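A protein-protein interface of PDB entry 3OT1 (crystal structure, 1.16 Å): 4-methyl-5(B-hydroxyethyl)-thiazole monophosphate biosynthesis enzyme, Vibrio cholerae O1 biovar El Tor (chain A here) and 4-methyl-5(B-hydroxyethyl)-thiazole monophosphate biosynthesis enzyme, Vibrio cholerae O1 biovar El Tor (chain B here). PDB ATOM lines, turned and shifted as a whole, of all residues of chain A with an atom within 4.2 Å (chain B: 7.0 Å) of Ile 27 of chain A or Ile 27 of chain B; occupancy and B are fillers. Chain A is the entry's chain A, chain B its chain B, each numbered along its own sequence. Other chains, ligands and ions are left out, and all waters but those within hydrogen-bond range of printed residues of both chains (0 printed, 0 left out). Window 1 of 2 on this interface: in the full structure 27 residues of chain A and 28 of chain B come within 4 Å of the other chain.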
ATOM      1  N   MET A  23      25.890 -10.087 -10.475  1.00  0.00           N
ATOM      2  CA  MET A  23      24.537 -10.589 -10.206  1.00  0.00           C
ATOM      3  C   MET A  23      24.215 -10.417  -8.727  1.00  0.00           C
ATOM      4  O   MET A  23      23.083 -10.083  -8.387  1.00  0.00           O
ATOM      5  CB  MET A  23      24.263 -12.004 -10.717  1.00  0.00           C
ATOM      6  CG  MET A  23      24.639 -13.137  -9.821  1.00  0.00           C
ATOM      7  SD  MET A  23      24.204 -14.825 -10.675  1.00  0.00           S
ATOM      8  CE  MET A  23      22.821 -15.621  -9.534  1.00  0.00           C
ATOM      9  N   GLU A  24      25.182 -10.638  -7.845  1.00  0.00           N
ATOM     10  CA  GLU A  24      24.914 -10.354  -6.440  1.00  0.00           C
ATOM     11  C   GLU A  24      24.518  -8.896  -6.241  1.00  0.00           C
ATOM     12  O   GLU A  24      23.569  -8.571  -5.543  1.00  0.00           O
ATOM     13  CB  GLU A  24      26.140 -10.683  -5.590  1.00  0.00           C
ATOM     14  CG  GLU A  24      26.492 -12.156  -5.572  1.00  0.00           C
ATOM     15  CD  GLU A  24      27.808 -12.482  -4.897  1.00  0.00           C
ATOM     16  OE1 GLU A  24      28.418 -11.621  -4.247  1.00  0.00           O
ATOM     17  OE2 GLU A  24      28.239 -13.672  -5.052  1.00  0.00           O
ATOM     18  N   THR A  25      25.303  -8.006  -6.828  1.00  0.00           N
ATOM     19  CA  THR A  25      25.057  -6.580  -6.712  1.00  0.00           C
ATOM     20  C   THR A  25      23.659  -6.214  -7.189  1.00  0.00           C
ATOM     21  O   THR A  25      22.924  -5.511  -6.495  1.00  0.00           O
ATOM     22  CB  THR A  25      26.105  -5.779  -7.526  1.00  0.00           C
ATOM     23  OG1 THR A  25      27.423  -6.066  -7.037  1.00  0.00           O
ATOM     24  CG2 THR A  25      25.856  -4.288  -7.414  1.00  0.00           C
ATOM     25  N   VAL A  26      23.306  -6.650  -8.386  1.00  0.00           N
ATOM     26  CA  VAL A  26      22.062  -6.239  -8.997  1.00  0.00           C
ATOM     27  C   VAL A  26      20.871  -6.911  -8.308  1.00  0.00           C
ATOM     28  O   VAL A  26      19.826  -6.291  -8.156  1.00  0.00           O
ATOM     29  CB  VAL A  26      22.109  -6.448 -10.521  1.00  0.00           C
ATOM     30  CG1 VAL A  26      20.760  -6.156 -11.133  1.00  0.00           C
ATOM     31  CG2 VAL A  26      23.182  -5.562 -11.125  1.00  0.00           C
ATOM     32  N   ILE A  27      21.021  -8.150  -7.859  1.00  0.00           N
ATOM     33  CA  ILE A  27      19.972  -8.775  -7.057  1.00  0.00           C
ATOM     34  C   ILE A  27      19.701  -7.946  -5.807  1.00  0.00           C
ATOM     35  O   ILE A  27      18.544  -7.701  -5.451  1.00  0.00           O
ATOM     36  CB  ILE A  27      20.306 -10.233  -6.706  1.00  0.00           C
ATOM     37  CG1 ILE A  27      20.245 -11.127  -7.952  1.00  0.00           C
ATOM     38  CG2 ILE A  27      19.368 -10.760  -5.570  1.00  0.00           C
ATOM     39  CD1 ILE A  27      20.875 -12.510  -7.774  1.00  0.00           C
ATOM     40  N   ILE A  28      20.752  -7.525  -5.121  1.00  0.00           N
ATOM     41  CA  ILE A  28      20.579  -6.708  -3.920  1.00  0.00           C
ATOM     42  C   ILE A  28      19.860  -5.414  -4.260  1.00  0.00           C
ATOM     43  O   ILE A  28      18.875  -5.069  -3.606  1.00  0.00           O
ATOM     44  CB  ILE A  28      21.946  -6.435  -3.245  1.00  0.00           C
ATOM     45  CG1 ILE A  28      22.551  -7.731  -2.689  1.00  0.00           C
ATOM     46  CG2 ILE A  28      21.805  -5.371  -2.165  1.00  0.00           C
ATOM     47  CD1 ILE A  28      24.055  -7.693  -2.455  1.00  0.00           C
ATOM     48  N   VAL A  29      20.360  -4.683  -5.241  1.00  0.00           N
ATOM     49  CA  VAL A  29      19.785  -3.383  -5.539  1.00  0.00           C
ATOM     50  C   VAL A  29      18.316  -3.516  -5.965  1.00  0.00           C
ATOM     51  O   VAL A  29      17.448  -2.831  -5.461  1.00  0.00           O
ATOM     52  CB  VAL A  29      20.607  -2.658  -6.631  1.00  0.00           C
ATOM     53  CG1 VAL A  29      19.881  -1.413  -7.088  1.00  0.00           C
ATOM     54  CG2 VAL A  29      22.018  -2.319  -6.107  1.00  0.00           C
ATOM     55  N   ASP A  30      18.070  -4.399  -6.924  1.00  0.00           N
ATOM     56  CA  ASP A  30      16.730  -4.572  -7.497  1.00  0.00           C
ATOM     57  C   ASP A  30      15.747  -4.977  -6.398  1.00  0.00           C
ATOM     58  O   ASP A  30      14.677  -4.382  -6.249  1.00  0.00           O
ATOM     59  CB  ASP A  30      16.835  -5.607  -8.633  1.00  0.00           C
ATOM     60  CG  ASP A  30      15.574  -5.868  -9.389  1.00  0.00           C
ATOM     61  OD1 ASP A  30      14.466  -5.836  -8.847  1.00  0.00           O
ATOM     62  OD2 ASP A  30      15.753  -6.150 -10.602  1.00  0.00           O
ATOM     63  N   THR A  31      16.097  -5.982  -5.614  1.00  0.00           N
ATOM     64  CA  THR A  31      15.194  -6.469  -4.580  1.00  0.00           C
ATOM     65  C   THR A  31      14.868  -5.386  -3.569  1.00  0.00           C
ATOM     66  O   THR A  31      13.713  -5.222  -3.161  1.00  0.00           O
ATOM     67  CB  THR A  31      15.762  -7.738  -3.907  1.00  0.00           C
ATOM     68  OG1 THR A  31      15.987  -8.735  -4.914  1.00  0.00           O
ATOM     69  CG2 THR A  31      14.808  -8.319  -2.884  1.00  0.00           C
ATOM     70  N   ALA A 166      21.710 -14.924  -2.967  1.00  0.00           N
ATOM     71  CA  ALA A 166      21.622 -13.484  -2.957  1.00  0.00           C
ATOM     72  C   ALA A 166      20.176 -12.989  -2.790  1.00  0.00           C
ATOM     73  O   ALA A 166      19.937 -12.003  -2.113  1.00  0.00           O
ATOM     74  CB  ALA A 166      22.284 -12.871  -4.191  1.00  0.00           C
ATOM     75  N   LEU A 167      19.227 -13.645  -3.461  1.00  0.00           N
ATOM     76  CA  LEU A 167      17.835 -13.271  -3.308  1.00  0.00           C
ATOM     77  C   LEU A 167      17.357 -13.496  -1.859  1.00  0.00           C
ATOM     78  O   LEU A 167      16.710 -12.639  -1.250  1.00  0.00           O
ATOM     79  CB  LEU A 167      17.025 -14.056  -4.311  1.00  0.00           C
ATOM     80  CG  LEU A 167      15.555 -13.745  -4.406  1.00  0.00           C
ATOM     81  CD1 LEU A 167      15.316 -12.262  -4.461  1.00  0.00           C
ATOM     82  CD2 LEU A 167      14.952 -14.455  -5.627  1.00  0.00           C
ATOM     83  N   GLU B  21      14.271  -6.103 -17.047  1.00  0.00           N
ATOM     84  CA  GLU B  21      14.482  -6.546 -15.670  1.00  0.00           C
ATOM     85  C   GLU B  21      15.986  -6.797 -15.487  1.00  0.00           C
ATOM     86  O   GLU B  21      16.545  -7.712 -16.107  1.00  0.00           O
ATOM     87  CB  GLU B  21      13.635  -7.775 -15.347  1.00  0.00           C
ATOM     88  CG  GLU B  21      13.039  -7.729 -13.959  1.00  0.00           C
ATOM     89  CD  GLU B  21      14.057  -7.647 -12.871  1.00  0.00           C
ATOM     90  OE1 GLU B  21      13.746  -6.998 -11.829  1.00  0.00           O
ATOM     91  OE2 GLU B  21      15.168  -8.195 -13.052  1.00  0.00           O
ATOM     92  N   GLU B  22      16.628  -5.941 -14.709  1.00  0.00           N
ATOM     93  CA  GLU B  22      18.089  -5.970 -14.613  1.00  0.00           C
ATOM     94  C   GLU B  22      18.628  -7.174 -13.881  1.00  0.00           C
ATOM     95  O   GLU B  22      19.714  -7.640 -14.231  1.00  0.00           O
ATOM     96  CB  GLU B  22      18.633  -4.692 -13.970  1.00  0.00           C
ATOM     97  CG  GLU B  22      17.975  -4.301 -12.656  1.00  0.00           C
ATOM     98  CD  GLU B  22      16.824  -3.330 -12.864  1.00  0.00           C
ATOM     99  OE1 GLU B  22      15.746  -3.797 -13.305  1.00  0.00           O
ATOM    100  OE2 GLU B  22      16.959  -2.135 -12.573  1.00  0.00           O
ATOM    101  N   MET B  23      17.942  -7.688 -12.864  1.00  0.00           N
ATOM    102  CA  MET B  23      18.458  -8.889 -12.217  1.00  0.00           C
ATOM    103  C   MET B  23      18.310 -10.097 -13.148  1.00  0.00           C
ATOM    104  O   MET B  23      19.232 -10.891 -13.237  1.00  0.00           O
ATOM    105  CB  MET B  23      17.936  -9.092 -10.797  1.00  0.00           C
ATOM    106  CG  MET B  23      16.589  -9.633 -10.587  1.00  0.00           C
ATOM    107  SD  MET B  23      16.420  -9.920  -8.638  1.00  0.00           S
ATOM    108  CE  MET B  23      16.703 -11.867  -8.438  1.00  0.00           C
ATOM    109  N   GLU B  24      17.209 -10.219 -13.878  1.00  0.00           N
ATOM    110  CA  GLU B  24      17.110 -11.277 -14.854  1.00  0.00           C
ATOM    111  C   GLU B  24      18.244 -11.161 -15.867  1.00  0.00           C
ATOM    112  O   GLU B  24      18.916 -12.152 -16.182  1.00  0.00           O
ATOM    113  CB  GLU B  24      15.766 -11.239 -15.560  1.00  0.00           C
ATOM    114  CG  GLU B  24      14.575 -11.496 -14.634  1.00  0.00           C
ATOM    115  CD  GLU B  24      13.226 -11.277 -15.284  1.00  0.00           C
ATOM    116  OE1 GLU B  24      13.145 -11.208 -16.511  1.00  0.00           O
ATOM    117  OE2 GLU B  24      12.236 -11.161 -14.531  1.00  0.00           O
ATOM    118  N   THR B  25      18.446  -9.955 -16.399  1.00  0.00           N
ATOM    119  CA  THR B  25      19.475  -9.726 -17.401  1.00  0.00           C
ATOM    120  C   THR B  25      20.849 -10.120 -16.893  1.00  0.00           C
ATOM    121  O   THR B  25      21.590 -10.833 -17.557  1.00  0.00           O
ATOM    122  CB  THR B  25      19.485  -8.248 -17.831  1.00  0.00           C
ATOM    123  OG1 THR B  25      18.212  -7.866 -18.366  1.00  0.00           O
ATOM    124  CG2 THR B  25      20.534  -7.988 -18.865  1.00  0.00           C
ATOM    125  N   VAL B  26      21.214  -9.612 -15.733  1.00  0.00           N
ATOM    126  CA  VAL B  26      22.566  -9.800 -15.232  1.00  0.00           C
ATOM    127  C   VAL B  26      22.790 -11.238 -14.761  1.00  0.00           C
ATOM    128  O   VAL B  26      23.874 -11.793 -14.937  1.00  0.00           O
ATOM    129  CB  VAL B  26      22.931  -8.728 -14.190  1.00  0.00           C
ATOM    130  CG1 VAL B  26      24.284  -9.031 -13.556  1.00  0.00           C
ATOM    131  CG2 VAL B  26      22.910  -7.346 -14.836  1.00  0.00           C
ATOM    132  N   ILE B  27      21.783 -11.880 -14.192  1.00  0.00           N
ATOM    133  CA  ILE B  27      21.880 -13.319 -13.883  1.00  0.00           C
ATOM    134  C   ILE B  27      22.196 -14.104 -15.149  1.00  0.00           C
ATOM    135  O   ILE B  27      23.087 -14.950 -15.153  1.00  0.00           O
ATOM    136  CB  ILE B  27      20.646 -13.878 -13.178  1.00  0.00           C
ATOM    137  CG1 ILE B  27      20.501 -13.302 -11.756  1.00  0.00           C
ATOM    138  CG2 ILE B  27      20.673 -15.401 -13.129  1.00  0.00           C
ATOM    139  CD1 ILE B  27      19.142 -13.507 -11.117  1.00  0.00           C
ATOM    140  N   ILE B  28      21.478 -13.817 -16.225  1.00  0.00           N
ATOM    141  CA  ILE B  28      21.720 -14.497 -17.486  1.00  0.00           C
ATOM    142  C   ILE B  28      23.153 -14.245 -17.985  1.00  0.00           C
ATOM    143  O   ILE B  28      23.891 -15.178 -18.299  1.00  0.00           O
ATOM    144  CB  ILE B  28      20.654 -14.081 -18.539  1.00  0.00           C
ATOM    145  CG1 ILE B  28      19.258 -14.584 -18.169  1.00  0.00           C
ATOM    146  CG2 ILE B  28      21.109 -14.558 -19.912  1.00  0.00           C
ATOM    147  CD1 ILE B  28      18.151 -13.863 -18.902  1.00  0.00           C
ATOM    148  N   VAL B  29      23.539 -12.982 -18.085  1.00  0.00           N
ATOM    149  CA  VAL B  29      24.830 -12.652 -18.640  1.00  0.00           C
ATOM    150  C   VAL B  29      25.960 -13.275 -17.806  1.00  0.00           C
ATOM    151  O   VAL B  29      26.844 -13.903 -18.356  1.00  0.00           O
ATOM    152  CB  VAL B  29      25.013 -11.134 -18.811  1.00  0.00           C
ATOM    153  CG1 VAL B  29      26.435 -10.797 -19.188  1.00  0.00           C
ATOM    154  CG2 VAL B  29      24.013 -10.558 -19.825  1.00  0.00           C
ATOM    155  N   ASP B  30      25.926 -13.058 -16.505  1.00  0.00           N
ATOM    156  CA  ASP B  30      26.969 -13.536 -15.610  1.00  0.00           C
ATOM    157  C   ASP B  30      27.092 -15.052 -15.687  1.00  0.00           C
ATOM    158  O   ASP B  30      28.196 -15.605 -15.859  1.00  0.00           O
ATOM    159  CB  ASP B  30      26.610 -13.005 -14.212  1.00  0.00           C
ATOM    160  CG  ASP B  30      27.570 -13.357 -13.119  1.00  0.00           C
ATOM    161  OD1 ASP B  30      28.326 -14.334 -13.196  1.00  0.00           O
ATOM    162  OD2 ASP B  30      27.469 -12.641 -12.087  1.00  0.00           O
ATOM    163  N   THR B  31      25.967 -15.756 -15.599  1.00  0.00           N
ATOM    164  CA  THR B  31      25.991 -17.210 -15.607  1.00  0.00           C
ATOM    165  C   THR B  31      26.561 -17.741 -16.923  1.00  0.00           C
ATOM    166  O   THR B  31      27.356 -18.692 -16.930  1.00  0.00           O
ATOM    167  CB  THR B  31      24.614 -17.801 -15.287  1.00  0.00           C
ATOM    168  OG1 THR B  31      24.139 -17.287 -14.034  1.00  0.00           O
ATOM    169  CG2 THR B  31      24.651 -19.303 -15.187  1.00  0.00           C
ATOM    170  N   LEU B  32      26.176 -17.133 -18.040  1.00  0.00           N
ATOM    171  CA  LEU B  32      26.701 -17.571 -19.329  1.00  0.00           C
ATOM    172  C   LEU B  32      28.192 -17.263 -19.484  1.00  0.00           C
ATOM    173  O   LEU B  32      28.941 -18.074 -20.039  1.00  0.00           O
ATOM    174  CB  LEU B  32      25.864 -16.980 -20.447  1.00  0.00           C
ATOM    175  CG  LEU B  32      24.412 -17.433 -20.499  1.00  0.00           C
ATOM    176  CD1 LEU B  32      23.667 -16.641 -21.566  1.00  0.00           C
ATOM    177  CD2 LEU B  32      24.282 -18.924 -20.716  1.00  0.00           C
ATOM    178  N   VAL B  33      28.643 -16.115 -18.990  1.00  0.00           N
ATOM    179  CA  VAL B  33      30.060 -15.799 -19.009  1.00  0.00           C
ATOM    180  C   VAL B  33      30.850 -16.785 -18.142  1.00  0.00           C
ATOM    181  O   VAL B  33      31.964 -17.185 -18.512  1.00  0.00           O
ATOM    182  CB  VAL B  33      30.319 -14.331 -18.590  1.00  0.00           C
ATOM    183  CG1 VAL B  33      31.782 -14.063 -18.357  1.00  0.00           C
ATOM    184  CG2 VAL B  33      29.765 -13.383 -19.639  1.00  0.00           C
ATOM    185  N   ARG B  34      30.271 -17.228 -17.031  1.00  0.00           N
ATOM    186  CA  ARG B  34      30.898 -18.248 -16.200  1.00  0.00           C
ATOM    187  C   ARG B  34      31.143 -19.555 -16.959  1.00  0.00           C
ATOM    188  O   ARG B  34      32.055 -20.305 -16.595  1.00  0.00           O
ATOM    189  CB  ARG B  34      30.058 -18.532 -14.955  1.00  0.00           C
ATOM    190  CG  ARG B  34      30.180 -17.470 -13.867  1.00  0.00           C
ATOM    191  CD  ARG B  34      29.041 -17.553 -12.880  1.00  0.00           C
ATOM    192  NE  ARG B  34      29.211 -16.614 -11.759  1.00  0.00           N
ATOM    193  CZ  ARG B  34      29.695 -16.917 -10.558  1.00  0.00           C
ATOM    194  NH1 ARG B  34      30.086 -18.142 -10.248  1.00  0.00           N
ATOM    195  NH2 ARG B  34      29.786 -15.944  -9.647  1.00  0.00           N
ATOM    196  N   GLY B 162      10.652 -16.215 -13.798  1.00  0.00           N
ATOM    197  CA  GLY B 162      10.867 -15.003 -13.031  1.00  0.00           C
ATOM    198  C   GLY B 162      12.257 -14.872 -12.483  1.00  0.00           C
ATOM    199  O   GLY B 162      13.105 -15.695 -12.740  1.00  0.00           O
ATOM    200  N   PRO B 163      12.501 -13.800 -11.732  1.00  0.00           N
ATOM    201  CA  PRO B 163      13.829 -13.593 -11.138  1.00  0.00           C
ATOM    202  C   PRO B 163      14.369 -14.809 -10.379  1.00  0.00           C
ATOM    203  O   PRO B 163      15.550 -15.143 -10.501  1.00  0.00           O
ATOM    204  CB  PRO B 163      13.615 -12.381 -10.234  1.00  0.00           C
ATOM    205  CG  PRO B 163      12.490 -11.631 -10.915  1.00  0.00           C
ATOM    206  CD  PRO B 163      11.576 -12.693 -11.415  1.00  0.00           C
ATOM    207  N   GLY B 164      13.478 -15.464  -9.633  1.00  0.00           N
ATOM    208  CA  GLY B 164      13.848 -16.618  -8.831  1.00  0.00           C
ATOM    209  C   GLY B 164      14.070 -17.899  -9.596  1.00  0.00           C
ATOM    210  O   GLY B 164      14.484 -18.894  -9.010  1.00  0.00           O
ATOM    211  N   THR B 165      13.766 -17.886 -10.904  1.00  0.00           N
ATOM    212  CA  THR B 165      14.077 -19.003 -11.782  1.00  0.00           C
ATOM    213  C   THR B 165      15.178 -18.670 -12.790  1.00  0.00           C
ATOM    214  O   THR B 165      15.530 -19.520 -13.611  1.00  0.00           O
ATOM    215  CB  THR B 165      12.824 -19.501 -12.568  1.00  0.00           C
ATOM    216  OG1 THR B 165      12.432 -18.551 -13.559  1.00  0.00           O
ATOM    217  CG2 THR B 165      11.663 -19.822 -11.678  1.00  0.00           C
ATOM    218  N   ALA B 166      15.757 -17.475 -12.733  1.00  0.00           N
ATOM    219  CA  ALA B 166      16.679 -17.033 -13.759  1.00  0.00           C
ATOM    220  C   ALA B 166      17.975 -17.845 -13.750  1.00  0.00           C
ATOM    221  O   ALA B 166      18.527 -18.137 -14.817  1.00  0.00           O
ATOM    222  CB  ALA B 166      16.949 -15.545 -13.641  1.00  0.00           C
ATOM    223  N   LEU B 167      18.493 -18.198 -12.572  1.00  0.00           N
ATOM    224  CA  LEU B 167      19.685 -19.016 -12.507  1.00  0.00           C
ATOM    225  C   LEU B 167      19.408 -20.415 -13.101  1.00  0.00           C
ATOM    226  O   LEU B 167      20.189 -20.918 -13.908  1.00  0.00           O
ATOM    227  CB  LEU B 167      20.157 -19.051 -11.068  1.00  0.00           C
ATOM    228  CG  LEU B 167      21.442 -19.771 -10.760  1.00  0.00           C
ATOM    229  CD1 LEU B 167      22.573 -19.391 -11.707  1.00  0.00           C
ATOM    230  CD2 LEU B 167      21.820 -19.466  -9.322  1.00  0.00           C
ATOM    231  N   GLU B 168      18.283 -21.027 -12.728  1.00  0.00           N
ATOM    232  CA  GLU B 168      17.886 -22.304 -13.295  1.00  0.00           C
ATOM    233  C   GLU B 168      17.793 -22.231 -14.815  1.00  0.00           C
ATOM    234  O   GLU B 168      18.220 -23.130 -15.519  1.00  0.00           O
ATOM    235  CB  GLU B 168      16.532 -22.733 -12.722  1.00  0.00           C
ATOM    236  CG  GLU B 168      16.557 -23.069 -11.239  1.00  0.00           C
ATOM    237  CD  GLU B 168      15.205 -22.857 -10.602  1.00  0.00           C
ATOM    238  OE1 GLU B 168      14.247 -23.598 -10.935  1.00  0.00           O
ATOM    239  OE2 GLU B 168      15.060 -21.959  -9.741  1.00  0.00           O
ATOM    240  N   ALA B 170      19.309 -20.006 -16.920  1.00  0.00           N
ATOM    241  CA  ALA B 170      20.606 -19.818 -17.566  1.00  0.00           C
ATOM    242  C   ALA B 170      21.391 -21.124 -17.548  1.00  0.00           C
ATOM    243  O   ALA B 170      22.077 -21.452 -18.516  1.00  0.00           O
ATOM    244  CB  ALA B 170      21.389 -18.694 -16.886  1.00  0.00           C
ATOM    245  N   MET B 190      28.141 -22.012  -7.036  1.00  0.00           N
ATOM    246  CA  MET B 190      27.233 -20.863  -6.955  1.00  0.00           C
ATOM    247  C   MET B 190      26.248 -20.876  -5.798  1.00  0.00           C
ATOM    248  O   MET B 190      25.559 -19.882  -5.592  1.00  0.00           O
ATOM    249  CB  MET B 190      26.488 -20.699  -8.285  1.00  0.00           C
ATOM    250  CG  MET B 190      27.435 -20.418  -9.450  1.00  0.00           C
ATOM    251  SD  MET B 190      26.561 -20.160 -11.161  1.00  0.00           S
ATOM    252  CE  MET B 190      25.930 -18.499 -10.795  1.00  0.00           C
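The side-chain carboxylate (OD2) of Asp 30 of chain B sits at hydrogen-bond distance from the backbone NH (N) of Met 23 of chain A, 3.4 Å away.
The side-chain carboxylate (OE1) of Glu 21 of chain B sits close to the side-chain carboxylate (OD2) of Asp 30 of chain A (2.5 Å).
The side-chain hydroxyl of Thr 31 of chain A is in hydrogen-bond range of the backbone carbonyl oxygen of Ile 27 of chain A (2.8 Å).
The backbone NH (N) of Met 23 of chain B sits at hydrogen-bond distance from the side-chain carboxylate (OE2) of Glu 21 of chain B (2.8 Å).
The backbone NH of Glu 24 of chain B lies within hydrogen-bond range of the side-chain carboxylate of Glu 21 of chain B (3.0 Å).
O of Glu 21 of chain B lies within hydrogen-bond range of OG1 of Thr 25 of chain B, 2.8 Å away.
The backbone carbonyl oxygen (O) of Ile 27 of chain B sits at hydrogen-bond distance from the side-chain hydroxyl (OG1) of Thr 31 of chain B (2.8 Å).
The side-chain carboxylate of Asp 30 of chain B lies within salt-bridge range of the guanidinium group of Arg 34 of chain B, at 2.8 Å.
Among the printed residues, pairs that only touch across the chains: Asp 30 of chain A with Met 23 of chain B, Asp 30 of chain A with Glu 22 of chain B, Val 26 of chain A with Glu 22 of chain B, Met 23 of chain A with Val 26 of chain B, Val 26 of chain A with Met 23 of chain B, Ile 27 of chain A with Met 23 of chain B, Ile 27 of chain A with Ile 27 of chain B, Thr 31 of chain A with Met 23 of chain B, Met 23 of chain A with Ile 27 of chain B and Met 23 of chain A with Leu 167 of chain B.
Of the printed residues of chain B, Val 26 of chain A touches Glu 22 and Met 23.
Of the printed residues of chain B, Asp 30 of chain A touches Glu 21 (2.5 Å), Glu 22 (3.5 Å) and Met 23 (3.5 Å).
Printed residues of chain B within 4 Å of Thr 31 of chain A: Met 23.
Printed residues of chain A within 4 Å of Met 23 of chain B: Val 26 (3.6 Å), Ile 27 (3.7 Å), Asp 30 (3.5 Å) and Thr 31 (3.9 Å).
Of the printed residues of chain A, Ile 27 of chain B touches Met 23 and Ile 27.
Of the printed residues of chain A, Leu 167 of chain B touches Met 23 (3.98 Å).
Of the 23 printed residues of chain B, 7 touch a printed residue of chain A.
Hydrophobic or aromatic side chains of chain B within 4 Å of the printed part of chain A: Met 23, Val 26, Ile 27 and Leu 167.
Of the 11 printed residues of chain A, 5 touch a printed residue of chain B.
Printed residues of chain A that touch a printed residue of chain B: Met 23, Val 26, Ile 27, Asp 30 and Thr 31.
Among the printed residues, 12 pairs touch across the chains.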
